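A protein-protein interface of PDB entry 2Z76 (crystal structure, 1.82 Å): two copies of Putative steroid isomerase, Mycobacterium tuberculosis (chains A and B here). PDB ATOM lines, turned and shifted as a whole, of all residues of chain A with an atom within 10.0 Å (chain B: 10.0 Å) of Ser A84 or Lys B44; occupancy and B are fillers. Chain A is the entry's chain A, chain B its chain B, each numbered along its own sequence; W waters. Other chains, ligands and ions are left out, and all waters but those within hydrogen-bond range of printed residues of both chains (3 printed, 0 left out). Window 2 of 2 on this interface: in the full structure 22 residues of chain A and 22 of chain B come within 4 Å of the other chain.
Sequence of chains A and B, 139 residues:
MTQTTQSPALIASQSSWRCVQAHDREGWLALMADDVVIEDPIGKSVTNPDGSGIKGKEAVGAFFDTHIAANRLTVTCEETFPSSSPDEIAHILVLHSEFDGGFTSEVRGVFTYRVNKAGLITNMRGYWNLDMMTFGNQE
N of Trp B128 sits at hydrogen-bond distance from O of Pro A82.
ND2 of Asn B129 sits at hydrogen-bond distance from O of Ser A83, at 3.1 Å.
The backbone NH of Ser A84 lies within hydrogen-bond range of the backbone carbonyl oxygen of Ile B42 (2.8 Å).
The backbone carbonyl oxygen (O) of Trp B128 sits at hydrogen-bond distance from the side-chain hydroxyl (OG) of Ser A84, at 2.9 Å.
The backbone NH (N) of Ser A85 sits at hydrogen-bond distance from the backbone carbonyl oxygen (O) of Ile B42 (3.4 Å).
OE1 of Glu A88 lies within salt-bridge range of NH1 of Arg B125.
O of Pro A82 sits close to O of Tyr B127, at 3.4 Å.
The side-chain sulfur (SD) of Met B132 sits close to the backbone carbonyl oxygen (O) of Pro A82 (3.8 Å).
N of Phe A81 sits at hydrogen-bond distance from O of Ala A90 (2.7 Å).
The side-chain hydroxyl of Ser A83 is in hydrogen-bond range of the backbone NH of Ser A85 (2.9 Å).
OG of Ser A85 lies close to N of Asp A87 (3.1 Å).
OE1 of Glu B39 is in salt-bridge range of NE of Arg B125.
OD1 of Asn B129 is in hydrogen-bond range of N of Asp B131 (2.9 Å).
OD1 of Asn B129 lies within hydrogen-bond range of N of Met B132, 3.1 Å away.
CB of Tyr B127 touches O of Phe A81 (3.6 Å).
Pro A82 touches Asn B129 (CB to ND2, 3.6 Å).
Ile B42 touches Ser A83.
Ser A84 touches Pro B41 (OG to CG, 3.3 Å).
Gly B43 touches Ser A84 (CA to C, 3.7 Å).
CB of Asn B129 touches OG of Ser A84, at 3.3 Å.
Ser A85 touches Gly B43.
Ile B42 touches Glu A88.
CE1 of Tyr B127 touches C of Ile A89 (3.6 Å).
Ala A90 touches Tyr B127 (N to CD1, 3.6 Å).
Ala A9 touches none of the printed residues of chain B.
Printed residues of chain B within 4 Å of Phe A81: Val B110 (3.3 Å) and Tyr B127 (3.6 Å).
Of chain B, only Ile B42, Tyr B127, Trp B128 and Asn B129 come within 4 Å of Ser A83.
Printed residues of chain B within 4 Å of Ser A84: Pro B41 (3.3 Å), Ile B42 (2.8 Å), Gly B43 (3.7 Å), Lys B44 (3.3 Å), Trp B128 (2.9 Å) and Asn B129 (3.3 Å).
Ser A85 touches just these residues of chain B: Ile B42 (3.4 Å) and Gly B43 (3.8 Å).
Of the printed residues of chain B, Ala A90 touches Tyr B127 (3.6 Å).
Of the printed residues of chain A, Pro B41 touches Ser A84 (3.3 Å).
Gly B43 touches just these residues of chain A: Ser A84 and Ser A85.
Lys B44 touches just one residue of chain A: Ser A84.
No residue of chain A comes within 4 Å of Ser B45.
No residue of chain A comes within 4 Å of Asn B48.
Pro B49 touches none of the printed residues of chain A.
No residue of chain A comes within 4 Å of Gly B51.
Printed residues of chain A within 4 Å of Arg B125: Glu A88 (3.0 Å).
Printed residues of chain A within 4 Å of Trp B128: Pro A82 (3.2 Å), Ser A83 (3.3 Å) and Ser A84 (2.9 Å).
The nearest residue of chain B that does not touch Ser A84 is Ser B45 (4.02 Å).
Printed residues of chain B that touch a printed residue of chain A: Pro B41, Ile B42, Gly B43, Lys B44, Val B110, Arg B125, Tyr B127, Trp B128, Asn B129 and Met B132.
Along chain B the printed residues that touch a printed residue of chain A span positions 41 to 132.
Of the 13 printed residues of chain A, 8 touch a printed residue of chain B.
Printed residues of chain A that touch a printed residue of chain B: Phe A81, Pro A82, Ser A83, Ser A84, Ser A85, Glu A88, Ile A89 and Ala A90.
No position is printed for both chains.
Of the 22 pairs that touch across the chains among the printed residues, none has its exchanged pair printed and touching as well.
Water W2 lies within hydrogen-bond range of the side-chain carboxylate of Glu A88 and the side-chain hydroxyl of Tyr B127.
Water W3 bridges O of Ser A84 (2.7 Å) and N of Lys B44 (2.9 Å).
Water W1 lies within hydrogen-bond range of OG of Ser B45, OG of Ser A84 and N of Leu B130.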
ATOM      1  N   SER A   7      -0.806 -11.615   6.398  1.00  0.00           N
ATOM      2  CA  SER A   7      -1.235 -10.220   6.244  1.00  0.00           C
ATOM      3  C   SER A   7      -0.922  -9.437   7.522  1.00  0.00           C
ATOM      4  O   SER A   7      -0.807 -10.047   8.590  1.00  0.00           O
ATOM      5  CB  SER A   7      -2.749 -10.134   5.971  1.00  0.00           C
ATOM      6  OG  SER A   7      -3.479 -10.478   7.137  1.00  0.00           O
ATOM      7  N   PRO A   8      -0.789  -8.108   7.417  1.00  0.00           N
ATOM      8  CA  PRO A   8      -0.654  -7.264   8.619  1.00  0.00           C
ATOM      9  C   PRO A   8      -1.775  -7.513   9.640  1.00  0.00           C
ATOM     10  O   PRO A   8      -1.508  -7.530  10.869  1.00  0.00           O
ATOM     11  CB  PRO A   8      -0.718  -5.837   8.062  1.00  0.00           C
ATOM     12  CG  PRO A   8      -0.225  -5.978   6.641  1.00  0.00           C
ATOM     13  CD  PRO A   8      -0.712  -7.309   6.175  1.00  0.00           C
ATOM     14  N   ALA A   9      -2.999  -7.699   9.163  1.00  0.00           N
ATOM     15  CA  ALA A   9      -4.144  -7.912  10.097  1.00  0.00           C
ATOM     16  C   ALA A   9      -3.976  -9.252  10.808  1.00  0.00           C
ATOM     17  O   ALA A   9      -4.231  -9.361  12.006  1.00  0.00           O
ATOM     18  CB  ALA A   9      -5.472  -7.854   9.366  1.00  0.00           C
ATOM     19  N   PHE A  81     -11.258 -15.547   9.089  1.00  0.00           N
ATOM     20  CA  PHE A  81     -11.948 -15.107   7.901  1.00  0.00           C
ATOM     21  C   PHE A  81     -11.249 -13.852   7.369  1.00  0.00           C
ATOM     22  O   PHE A  81     -11.557 -12.729   7.827  1.00  0.00           O
ATOM     23  CB  PHE A  81     -13.405 -14.794   8.248  1.00  0.00           C
ATOM     24  CG  PHE A  81     -14.257 -16.013   8.547  1.00  0.00           C
ATOM     25  CD1 PHE A  81     -14.938 -16.657   7.518  1.00  0.00           C
ATOM     26  CD2 PHE A  81     -14.417 -16.491   9.856  1.00  0.00           C
ATOM     27  CE1 PHE A  81     -15.760 -17.764   7.760  1.00  0.00           C
ATOM     28  CE2 PHE A  81     -15.240 -17.613  10.098  1.00  0.00           C
ATOM     29  CZ  PHE A  81     -15.906 -18.235   9.054  1.00  0.00           C
ATOM     30  N   PRO A  82     -10.288 -14.030   6.439  1.00  0.00           N
ATOM     31  CA  PRO A  82      -9.635 -12.907   5.756  1.00  0.00           C
ATOM     32  C   PRO A  82     -10.722 -12.092   5.030  1.00  0.00           C
ATOM     33  O   PRO A  82     -11.792 -12.628   4.772  1.00  0.00           O
ATOM     34  CB  PRO A  82      -8.731 -13.610   4.724  1.00  0.00           C
ATOM     35  CG  PRO A  82      -8.496 -14.986   5.300  1.00  0.00           C
ATOM     36  CD  PRO A  82      -9.805 -15.343   5.922  1.00  0.00           C
ATOM     37  N   SER A  83     -10.453 -10.824   4.757  1.00  0.00           N
ATOM     38  CA  SER A  83     -11.302 -10.012   3.887  1.00  0.00           C
ATOM     39  C   SER A  83     -10.491  -9.850   2.607  1.00  0.00           C
ATOM     40  O   SER A  83      -9.547 -10.655   2.363  1.00  0.00           O
ATOM     41  CB  SER A  83     -11.597  -8.652   4.536  1.00  0.00           C
ATOM     42  OG  SER A  83     -10.447  -7.816   4.557  1.00  0.00           O
ATOM     43  N   SER A  84     -10.841  -8.851   1.776  1.00  0.00           N
ATOM     44  CA  SER A  84     -10.019  -8.529   0.588  1.00  0.00           C
ATOM     45  C   SER A  84      -9.064  -7.382   0.871  1.00  0.00           C
ATOM     46  O   SER A  84      -8.373  -6.883  -0.042  1.00  0.00           O
ATOM     47  CB  SER A  84     -10.901  -8.287  -0.661  1.00  0.00           C
ATOM     48  OG  SER A  84     -11.696  -9.425  -0.906  1.00  0.00           O
ATOM     49  N   SER A  85      -9.020  -6.954   2.148  1.00  0.00           N
ATOM     50  CA  SER A  85      -8.062  -5.956   2.603  1.00  0.00           C
ATOM     51  C   SER A  85      -7.056  -6.695   3.475  1.00  0.00           C
ATOM     52  O   SER A  85      -7.476  -7.406   4.393  1.00  0.00           O
ATOM     53  CB  SER A  85      -8.735  -4.888   3.472  1.00  0.00           C
ATOM     54  OG  SER A  85      -7.738  -4.048   3.994  1.00  0.00           O
ATOM     55  N   PRO A  86      -5.745  -6.550   3.204  1.00  0.00           N
ATOM     56  CA  PRO A  86      -4.745  -7.177   4.089  1.00  0.00           C
ATOM     57  C   PRO A  86      -4.797  -6.560   5.506  1.00  0.00           C
ATOM     58  O   PRO A  86      -4.149  -7.065   6.427  1.00  0.00           O
ATOM     59  CB  PRO A  86      -3.406  -6.757   3.465  1.00  0.00           C
ATOM     60  CG  PRO A  86      -3.737  -6.409   2.040  1.00  0.00           C
ATOM     61  CD  PRO A  86      -5.115  -5.838   2.066  1.00  0.00           C
ATOM     62  N   ASP A  87      -5.533  -5.456   5.640  1.00  0.00           N
ATOM     63  CA  ASP A  87      -5.588  -4.720   6.917  1.00  0.00           C
ATOM     64  C   ASP A  87      -6.820  -4.971   7.806  1.00  0.00           C
ATOM     65  O   ASP A  87      -6.919  -4.343   8.884  1.00  0.00           O
ATOM     66  CB  ASP A  87      -5.473  -3.223   6.658  1.00  0.00           C
ATOM     67  CG  ASP A  87      -4.106  -2.813   6.128  1.00  0.00           C
ATOM     68  OD1 ASP A  87      -3.133  -3.602   6.166  1.00  0.00           O
ATOM     69  OD2 ASP A  87      -3.998  -1.659   5.675  1.00  0.00           O
ATOM     70  N   GLU A  88      -7.738  -5.810   7.347  1.00  0.00           N
ATOM     71  CA  GLU A  88      -8.941  -6.203   8.091  1.00  0.00           C
ATOM     72  C   GLU A  88      -9.241  -7.699   8.038  1.00  0.00           C
ATOM     73  O   GLU A  88      -9.165  -8.350   6.973  1.00  0.00           O
ATOM     74  CB  GLU A  88     -10.176  -5.407   7.611  1.00  0.00           C
ATOM     75  CG  GLU A  88      -9.951  -3.897   7.717  1.00  0.00           C
ATOM     76  CD  GLU A  88     -11.240  -3.096   7.774  1.00  0.00           C
ATOM     77  OE1 GLU A  88     -12.087  -3.418   8.629  1.00  0.00           O
ATOM     78  OE2 GLU A  88     -11.389  -2.157   6.963  1.00  0.00           O
ATOM     79  N   ILE A  89      -9.653  -8.250   9.188  1.00  0.00           N
ATOM     80  CA  ILE A  89      -9.794  -9.689   9.323  1.00  0.00           C
ATOM     81  C   ILE A  89     -10.776  -9.944  10.446  1.00  0.00           C
ATOM     82  O   ILE A  89     -10.872  -9.105  11.369  1.00  0.00           O
ATOM     83  CB  ILE A  89      -8.403 -10.383   9.644  1.00  0.00           C
ATOM     84  CG1 ILE A  89      -8.471 -11.916   9.512  1.00  0.00           C
ATOM     85  CG2 ILE A  89      -7.804  -9.962  11.045  1.00  0.00           C
ATOM     86  CD1 ILE A  89      -7.093 -12.485   9.229  1.00  0.00           C
ATOM     87  N   ALA A  90     -11.453 -11.093  10.370  1.00  0.00           N
ATOM     88  CA  ALA A  90     -12.365 -11.514  11.433  1.00  0.00           C
ATOM     89  C   ALA A  90     -11.998 -12.924  11.874  1.00  0.00           C
ATOM     90  O   ALA A  90     -11.436 -13.708  11.098  1.00  0.00           O
ATOM     91  CB  ALA A  90     -13.815 -11.456  10.952  1.00  0.00           C
ATOM     92  N   GLU B  39     -19.817  -2.771   2.045  1.00  0.00           N
ATOM     93  CA  GLU B  39     -18.510  -3.256   1.650  1.00  0.00           C
ATOM     94  C   GLU B  39     -18.603  -4.765   1.565  1.00  0.00           C
ATOM     95  O   GLU B  39     -18.341  -5.466   2.535  1.00  0.00           O
ATOM     96  CB  GLU B  39     -17.456  -2.830   2.662  1.00  0.00           C
ATOM     97  CG  GLU B  39     -17.108  -1.335   2.666  1.00  0.00           C
ATOM     98  CD  GLU B  39     -16.365  -0.945   3.943  1.00  0.00           C
ATOM     99  OE1 GLU B  39     -17.047  -0.551   4.906  1.00  0.00           O
ATOM    100  OE2 GLU B  39     -15.118  -1.048   4.014  1.00  0.00           O
ATOM    101  N   ASP B  40     -18.981  -5.285   0.397  1.00  0.00           N
ATOM    102  CA  ASP B  40     -19.136  -6.711   0.250  1.00  0.00           C
ATOM    103  C   ASP B  40     -18.273  -7.211  -0.909  1.00  0.00           C
ATOM    104  O   ASP B  40     -18.737  -7.199  -2.059  1.00  0.00           O
ATOM    105  CB  ASP B  40     -20.610  -7.058   0.011  1.00  0.00           C
ATOM    106  CG  ASP B  40     -20.874  -8.540   0.055  1.00  0.00           C
ATOM    107  OD1 ASP B  40     -19.945  -9.318   0.390  1.00  0.00           O
ATOM    108  OD2 ASP B  40     -22.022  -8.946  -0.235  1.00  0.00           O
ATOM    109  N   PRO B  41     -17.019  -7.624  -0.621  1.00  0.00           N
ATOM    110  CA  PRO B  41     -16.392  -7.730   0.715  1.00  0.00           C
ATOM    111  C   PRO B  41     -15.699  -6.428   1.092  1.00  0.00           C
ATOM    112  O   PRO B  41     -15.665  -5.489   0.286  1.00  0.00           O
ATOM    113  CB  PRO B  41     -15.315  -8.785   0.492  1.00  0.00           C
ATOM    114  CG  PRO B  41     -14.825  -8.450  -0.950  1.00  0.00           C
ATOM    115  CD  PRO B  41     -16.049  -7.913  -1.697  1.00  0.00           C
ATOM    116  N   ILE B  42     -15.104  -6.371   2.294  1.00  0.00           N
ATOM    117  CA  ILE B  42     -14.164  -5.330   2.640  1.00  0.00           C
ATOM    118  C   ILE B  42     -12.892  -5.437   1.800  1.00  0.00           C
ATOM    119  O   ILE B  42     -12.321  -6.516   1.716  1.00  0.00           O
ATOM    120  CB  ILE B  42     -13.736  -5.467   4.153  1.00  0.00           C
ATOM    121  CG1 ILE B  42     -14.981  -5.269   5.049  1.00  0.00           C
ATOM    122  CG2 ILE B  42     -12.606  -4.463   4.486  1.00  0.00           C
ATOM    123  CD1 ILE B  42     -14.886  -5.921   6.473  1.00  0.00           C
ATOM    124  N   GLY B  43     -12.441  -4.326   1.217  1.00  0.00           N
ATOM    125  CA  GLY B  43     -11.196  -4.333   0.446  1.00  0.00           C
ATOM    126  C   GLY B  43     -11.544  -4.496  -1.024  1.00  0.00           C
ATOM    127  O   GLY B  43     -12.698  -4.645  -1.363  1.00  0.00           O
ATOM    128  N   LYS B  44     -10.534  -4.453  -1.882  1.00  0.00           N
ATOM    129  CA  LYS B  44     -10.758  -4.423  -3.350  1.00  0.00           C
ATOM    130  C   LYS B  44     -11.151  -5.802  -3.898  1.00  0.00           C
ATOM    131  O   LYS B  44     -10.465  -6.812  -3.637  1.00  0.00           O
ATOM    132  CB  LYS B  44      -9.511  -3.895  -4.067  1.00  0.00           C
ATOM    133  CG  LYS B  44      -9.142  -2.486  -3.690  1.00  0.00           C
ATOM    134  CD  LYS B  44      -8.121  -1.861  -4.626  1.00  0.00           C
ATOM    135  CE  LYS B  44      -7.693  -0.498  -4.072  1.00  0.00           C
ATOM    136  NZ  LYS B  44      -6.739   0.210  -4.957  1.00  0.00           N
ATOM    137  N   SER B  45     -12.257  -5.852  -4.640  1.00  0.00           N
ATOM    138  CA  SER B  45     -12.717  -7.104  -5.251  1.00  0.00           C
ATOM    139  C   SER B  45     -13.663  -6.773  -6.392  1.00  0.00           C
ATOM    140  O   SER B  45     -13.951  -5.601  -6.652  1.00  0.00           O
ATOM    141  CB  SER B  45     -13.447  -8.010  -4.238  1.00  0.00           C
ATOM    142  OG  SER B  45     -13.465  -9.400  -4.633  1.00  0.00           O
ATOM    143  N   VAL B  46     -14.123  -7.826  -7.067  1.00  0.00           N
ATOM    144  CA  VAL B  46     -15.028  -7.691  -8.215  1.00  0.00           C
ATOM    145  C   VAL B  46     -16.288  -6.898  -7.815  1.00  0.00           C
ATOM    146  O   VAL B  46     -16.771  -6.029  -8.574  1.00  0.00           O
ATOM    147  CB  VAL B  46     -15.342  -9.048  -8.893  1.00  0.00           C
ATOM    148  CG1 VAL B  46     -16.323  -9.871  -8.073  1.00  0.00           C
ATOM    149  CG2 VAL B  46     -15.868  -8.818 -10.294  1.00  0.00           C
ATOM    150  N   THR B  47     -16.771  -7.161  -6.599  1.00  0.00           N
ATOM    151  CA  THR B  47     -17.977  -6.504  -6.111  1.00  0.00           C
ATOM    152  C   THR B  47     -17.710  -5.256  -5.245  1.00  0.00           C
ATOM    153  O   THR B  47     -18.664  -4.647  -4.742  1.00  0.00           O
ATOM    154  CB  THR B  47     -18.855  -7.491  -5.347  1.00  0.00           C
ATOM    155  OG1 THR B  47     -18.066  -8.142  -4.346  1.00  0.00           O
ATOM    156  CG2 THR B  47     -19.408  -8.546  -6.280  1.00  0.00           C
ATOM    157  N   ASN B  48     -16.439  -4.882  -5.079  1.00  0.00           N
ATOM    158  CA  ASN B  48     -16.004  -3.624  -4.421  1.00  0.00           C
ATOM    159  C   ASN B  48     -14.733  -3.134  -5.106  1.00  0.00           C
ATOM    160  O   ASN B  48     -13.627  -3.215  -4.555  1.00  0.00           O
ATOM    161  CB  ASN B  48     -15.767  -3.883  -2.903  1.00  0.00           C
ATOM    162  CG  ASN B  48     -15.515  -2.625  -2.105  1.00  0.00           C
ATOM    163  OD1 ASN B  48     -15.436  -1.522  -2.639  1.00  0.00           O
ATOM    164  ND2 ASN B  48     -15.375  -2.795  -0.775  1.00  0.00           N
ATOM    165  N   PRO B  49     -14.868  -2.648  -6.364  1.00  0.00           N
ATOM    166  CA  PRO B  49     -13.704  -2.435  -7.215  1.00  0.00           C
ATOM    167  C   PRO B  49     -12.601  -1.585  -6.618  1.00  0.00           C
ATOM    168  O   PRO B  49     -11.416  -1.968  -6.695  1.00  0.00           O
ATOM    169  CB  PRO B  49     -14.324  -1.792  -8.471  1.00  0.00           C
ATOM    170  CG  PRO B  49     -15.671  -2.393  -8.525  1.00  0.00           C
ATOM    171  CD  PRO B  49     -16.123  -2.365  -7.083  1.00  0.00           C
ATOM    172  N   ASP B  50     -12.962  -0.467  -5.993  1.00  0.00           N
ATOM    173  CA  ASP B  50     -11.922   0.403  -5.404  1.00  0.00           C
ATOM    174  C   ASP B  50     -11.757   0.276  -3.891  1.00  0.00           C
ATOM    175  O   ASP B  50     -11.003   1.022  -3.285  1.00  0.00           O
ATOM    176  CB  ASP B  50     -12.101   1.865  -5.817  1.00  0.00           C
ATOM    177  CG  ASP B  50     -13.323   2.536  -5.186  1.00  0.00           C
ATOM    178  OD1 ASP B  50     -13.943   1.998  -4.237  1.00  0.00           O
ATOM    179  OD2 ASP B  50     -13.663   3.641  -5.668  1.00  0.00           O
ATOM    180  N   GLY B  51     -12.433  -0.692  -3.296  1.00  0.00           N
ATOM    181  CA  GLY B  51     -12.279  -0.917  -1.865  1.00  0.00           C
ATOM    182  C   GLY B  51     -13.098   0.034  -0.995  1.00  0.00           C
ATOM    183  O   GLY B  51     -13.237  -0.212   0.191  1.00  0.00           O
ATOM    184  N   SER B  52     -13.682   1.086  -1.573  1.00  0.00           N
ATOM    185  CA  SER B  52     -14.405   2.110  -0.775  1.00  0.00           C
ATOM    186  C   SER B  52     -15.879   1.750  -0.521  1.00  0.00           C
ATOM    187  O   SER B  52     -16.589   2.454   0.213  1.00  0.00           O
ATOM    188  CB  SER B  52     -14.285   3.514  -1.429  1.00  0.00           C
ATOM    189  OG  SER B  52     -15.145   3.619  -2.560  1.00  0.00           O
ATOM    190  N   GLY B  53     -16.343   0.659  -1.112  1.00  0.00           N
ATOM    191  CA  GLY B  53     -17.697   0.184  -0.886  1.00  0.00           C
ATOM    192  C   GLY B  53     -18.753   0.816  -1.782  1.00  0.00           C
ATOM    193  O   GLY B  53     -18.466   1.769  -2.507  1.00  0.00           O
ATOM    194  N   VAL B 107     -19.286 -18.581  -1.622  1.00  0.00           N
ATOM    195  CA  VAL B 107     -18.287 -18.084  -0.690  1.00  0.00           C
ATOM    196  C   VAL B 107     -18.879 -18.057   0.724  1.00  0.00           C
ATOM    197  O   VAL B 107     -20.048 -17.751   0.902  1.00  0.00           O
ATOM    198  CB  VAL B 107     -17.750 -16.689  -1.119  1.00  0.00           C
ATOM    199  CG1 VAL B 107     -18.767 -15.573  -0.811  1.00  0.00           C
ATOM    200  CG2 VAL B 107     -16.369 -16.412  -0.489  1.00  0.00           C
ATOM    201  N   VAL B 110     -17.697 -13.987   7.177  1.00  0.00           N
ATOM    202  CA  VAL B 110     -18.357 -13.300   8.295  1.00  0.00           C
ATOM    203  C   VAL B 110     -18.931 -12.003   7.731  1.00  0.00           C
ATOM    204  O   VAL B 110     -18.261 -11.300   6.969  1.00  0.00           O
ATOM    205  CB  VAL B 110     -17.333 -12.956   9.414  1.00  0.00           C
ATOM    206  CG1 VAL B 110     -17.931 -11.965  10.403  1.00  0.00           C
ATOM    207  CG2 VAL B 110     -16.866 -14.250  10.140  1.00  0.00           C
ATOM    208  N   ARG B 125     -20.676  -5.236   5.994  1.00  0.00           N
ATOM    209  CA  ARG B 125     -19.239  -5.448   5.729  1.00  0.00           C
ATOM    210  C   ARG B 125     -18.947  -6.946   5.729  1.00  0.00           C
ATOM    211  O   ARG B 125     -19.323  -7.672   6.671  1.00  0.00           O
ATOM    212  CB  ARG B 125     -18.375  -4.753   6.787  1.00  0.00           C
ATOM    213  CG  ARG B 125     -18.783  -3.303   7.078  1.00  0.00           C
ATOM    214  CD  ARG B 125     -17.728  -2.610   7.918  1.00  0.00           C
ATOM    215  NE  ARG B 125     -16.601  -2.152   7.102  1.00  0.00           N
ATOM    216  CZ  ARG B 125     -15.327  -2.384   7.399  1.00  0.00           C
ATOM    217  NH1 ARG B 125     -15.022  -3.017   8.520  1.00  0.00           N
ATOM    218  NH2 ARG B 125     -14.356  -1.919   6.629  1.00  0.00           N
ATOM    219  N   GLY B 126     -18.299  -7.410   4.666  1.00  0.00           N
ATOM    220  CA  GLY B 126     -18.092  -8.830   4.470  1.00  0.00           C
ATOM    221  C   GLY B 126     -16.626  -9.219   4.480  1.00  0.00           C
ATOM    222  O   GLY B 126     -15.792  -8.606   3.791  1.00  0.00           O
ATOM    223  N   TYR B 127     -16.299 -10.227   5.293  1.00  0.00           N
ATOM    224  CA  TYR B 127     -14.937 -10.732   5.395  1.00  0.00           C
ATOM    225  C   TYR B 127     -14.850 -11.972   4.528  1.00  0.00           C
ATOM    226  O   TYR B 127     -15.152 -13.096   4.959  1.00  0.00           O
ATOM    227  CB  TYR B 127     -14.544 -11.054   6.865  1.00  0.00           C
ATOM    228  CG  TYR B 127     -14.541  -9.820   7.736  1.00  0.00           C
ATOM    229  CD1 TYR B 127     -13.339  -9.159   8.043  1.00  0.00           C
ATOM    230  CD2 TYR B 127     -15.740  -9.305   8.250  1.00  0.00           C
ATOM    231  CE1 TYR B 127     -13.329  -8.023   8.811  1.00  0.00           C
ATOM    232  CE2 TYR B 127     -15.741  -8.189   9.042  1.00  0.00           C
ATOM    233  CZ  TYR B 127     -14.541  -7.552   9.333  1.00  0.00           C
ATOM    234  OH  TYR B 127     -14.502  -6.403  10.095  1.00  0.00           O
ATOM    235  N   TRP B 128     -14.496 -11.739   3.270  1.00  0.00           N
ATOM    236  CA  TRP B 128     -14.154 -12.830   2.377  1.00  0.00           C
ATOM    237  C   TRP B 128     -13.321 -12.268   1.222  1.00  0.00           C
ATOM    238  O   TRP B 128     -13.185 -11.036   1.056  1.00  0.00           O
ATOM    239  CB  TRP B 128     -15.422 -13.544   1.904  1.00  0.00           C
ATOM    240  CG  TRP B 128     -16.374 -12.689   1.130  1.00  0.00           C
ATOM    241  CD1 TRP B 128     -17.447 -11.968   1.629  1.00  0.00           C
ATOM    242  CD2 TRP B 128     -16.354 -12.452  -0.282  1.00  0.00           C
ATOM    243  NE1 TRP B 128     -18.099 -11.311   0.604  1.00  0.00           N
ATOM    244  CE2 TRP B 128     -17.459 -11.597  -0.582  1.00  0.00           C
ATOM    245  CE3 TRP B 128     -15.541 -12.915  -1.332  1.00  0.00           C
ATOM    246  CZ2 TRP B 128     -17.749 -11.177  -1.890  1.00  0.00           C
ATOM    247  CZ3 TRP B 128     -15.821 -12.496  -2.636  1.00  0.00           C
ATOM    248  CH2 TRP B 128     -16.907 -11.629  -2.901  1.00  0.00           C
ATOM    249  N   ASN B 129     -12.716 -13.181   0.452  1.00  0.00           N
ATOM    250  CA  ASN B 129     -11.999 -12.769  -0.751  1.00  0.00           C
ATOM    251  C   ASN B 129     -12.175 -13.869  -1.839  1.00  0.00           C
ATOM    252  O   ASN B 129     -12.786 -14.932  -1.575  1.00  0.00           O
ATOM    253  CB  ASN B 129     -10.532 -12.436  -0.436  1.00  0.00           C
ATOM    254  CG  ASN B 129      -9.742 -13.635   0.106  1.00  0.00           C
ATOM    255  OD1 ASN B 129      -9.788 -14.730  -0.457  1.00  0.00           O
ATOM    256  ND2 ASN B 129      -8.998 -13.418   1.187  1.00  0.00           N
ATOM    257  N   LEU B 130     -11.704 -13.582  -3.052  1.00  0.00           N
ATOM    258  CA  LEU B 130     -11.868 -14.525  -4.160  1.00  0.00           C
ATOM    259  C   LEU B 130     -11.012 -15.777  -4.017  1.00  0.00           C
ATOM    260  O   LEU B 130     -11.343 -16.808  -4.627  1.00  0.00           O
ATOM    261  CB  LEU B 130     -11.556 -13.847  -5.508  1.00  0.00           C
ATOM    262  CG  LEU B 130     -12.480 -12.709  -5.911  1.00  0.00           C
ATOM    263  CD1 LEU B 130     -11.816 -11.862  -6.995  1.00  0.00           C
ATOM    264  CD2 LEU B 130     -13.833 -13.222  -6.371  1.00  0.00           C
ATOM    265  N   ASP B 131      -9.932 -15.706  -3.233  1.00  0.00           N
ATOM    266  CA  ASP B 131      -9.131 -16.923  -2.920  1.00  0.00           C
ATOM    267  C   ASP B 131      -9.949 -17.917  -2.122  1.00  0.00           C
ATOM    268  O   ASP B 131      -9.673 -19.114  -2.167  1.00  0.00           O
ATOM    269  CB  ASP B 131      -7.835 -16.628  -2.162  1.00  0.00           C
ATOM    270  CG  ASP B 131      -6.850 -15.787  -2.961  1.00  0.00           C
ATOM    271  OD1 ASP B 131      -6.704 -16.022  -4.178  1.00  0.00           O
ATOM    272  OD2 ASP B 131      -6.224 -14.868  -2.354  1.00  0.00           O
ATOM    273  N   MET B 132     -10.959 -17.423  -1.401  1.00  0.00           N
ATOM    274  CA  MET B 132     -11.854 -18.258  -0.596  1.00  0.00           C
ATOM    275  C   MET B 132     -13.049 -18.763  -1.357  1.00  0.00           C
ATOM    276  O   MET B 132     -13.808 -19.587  -0.855  1.00  0.00           O
ATOM    277  CB  MET B 132     -12.390 -17.481   0.613  1.00  0.00           C
ATOM    278  CG  MET B 132     -11.347 -17.168   1.640  1.00  0.00           C
ATOM    279  SD  MET B 132     -11.864 -15.752   2.653  1.00  0.00           S
ATOM    280  CE  MET B 132     -13.233 -16.395   3.595  1.00  0.00           C
ATOM    281  N   MET B 133     -13.246 -18.245  -2.563  1.00  0.00           N
ATOM    282  CA  MET B 133     -14.443 -18.555  -3.323  1.00  0.00           C
ATOM    283  C   MET B 133     -14.311 -19.882  -4.082  1.00  0.00           C
ATOM    284  O   MET B 133     -13.216 -20.251  -4.520  1.00  0.00           O
ATOM    285  CB  MET B 133     -14.751 -17.409  -4.281  1.00  0.00           C
ATOM    286  CG  MET B 133     -16.079 -17.489  -4.964  1.00  0.00           C
ATOM    287  SD  MET B 133     -16.476 -15.954  -5.832  1.00  0.00           S
ATOM    288  CE  MET B 133     -17.581 -15.200  -4.640  1.00  0.00           C
HETATM  289  O   HOH W   1     -11.285 -10.628  -3.411  1.00  0.00           O
HETATM  290  O   HOH W   2     -12.159  -5.099  10.617  1.00  0.00           O
HETATM  291  O   HOH W   3      -7.825  -4.362  -0.810  1.00  0.00           O
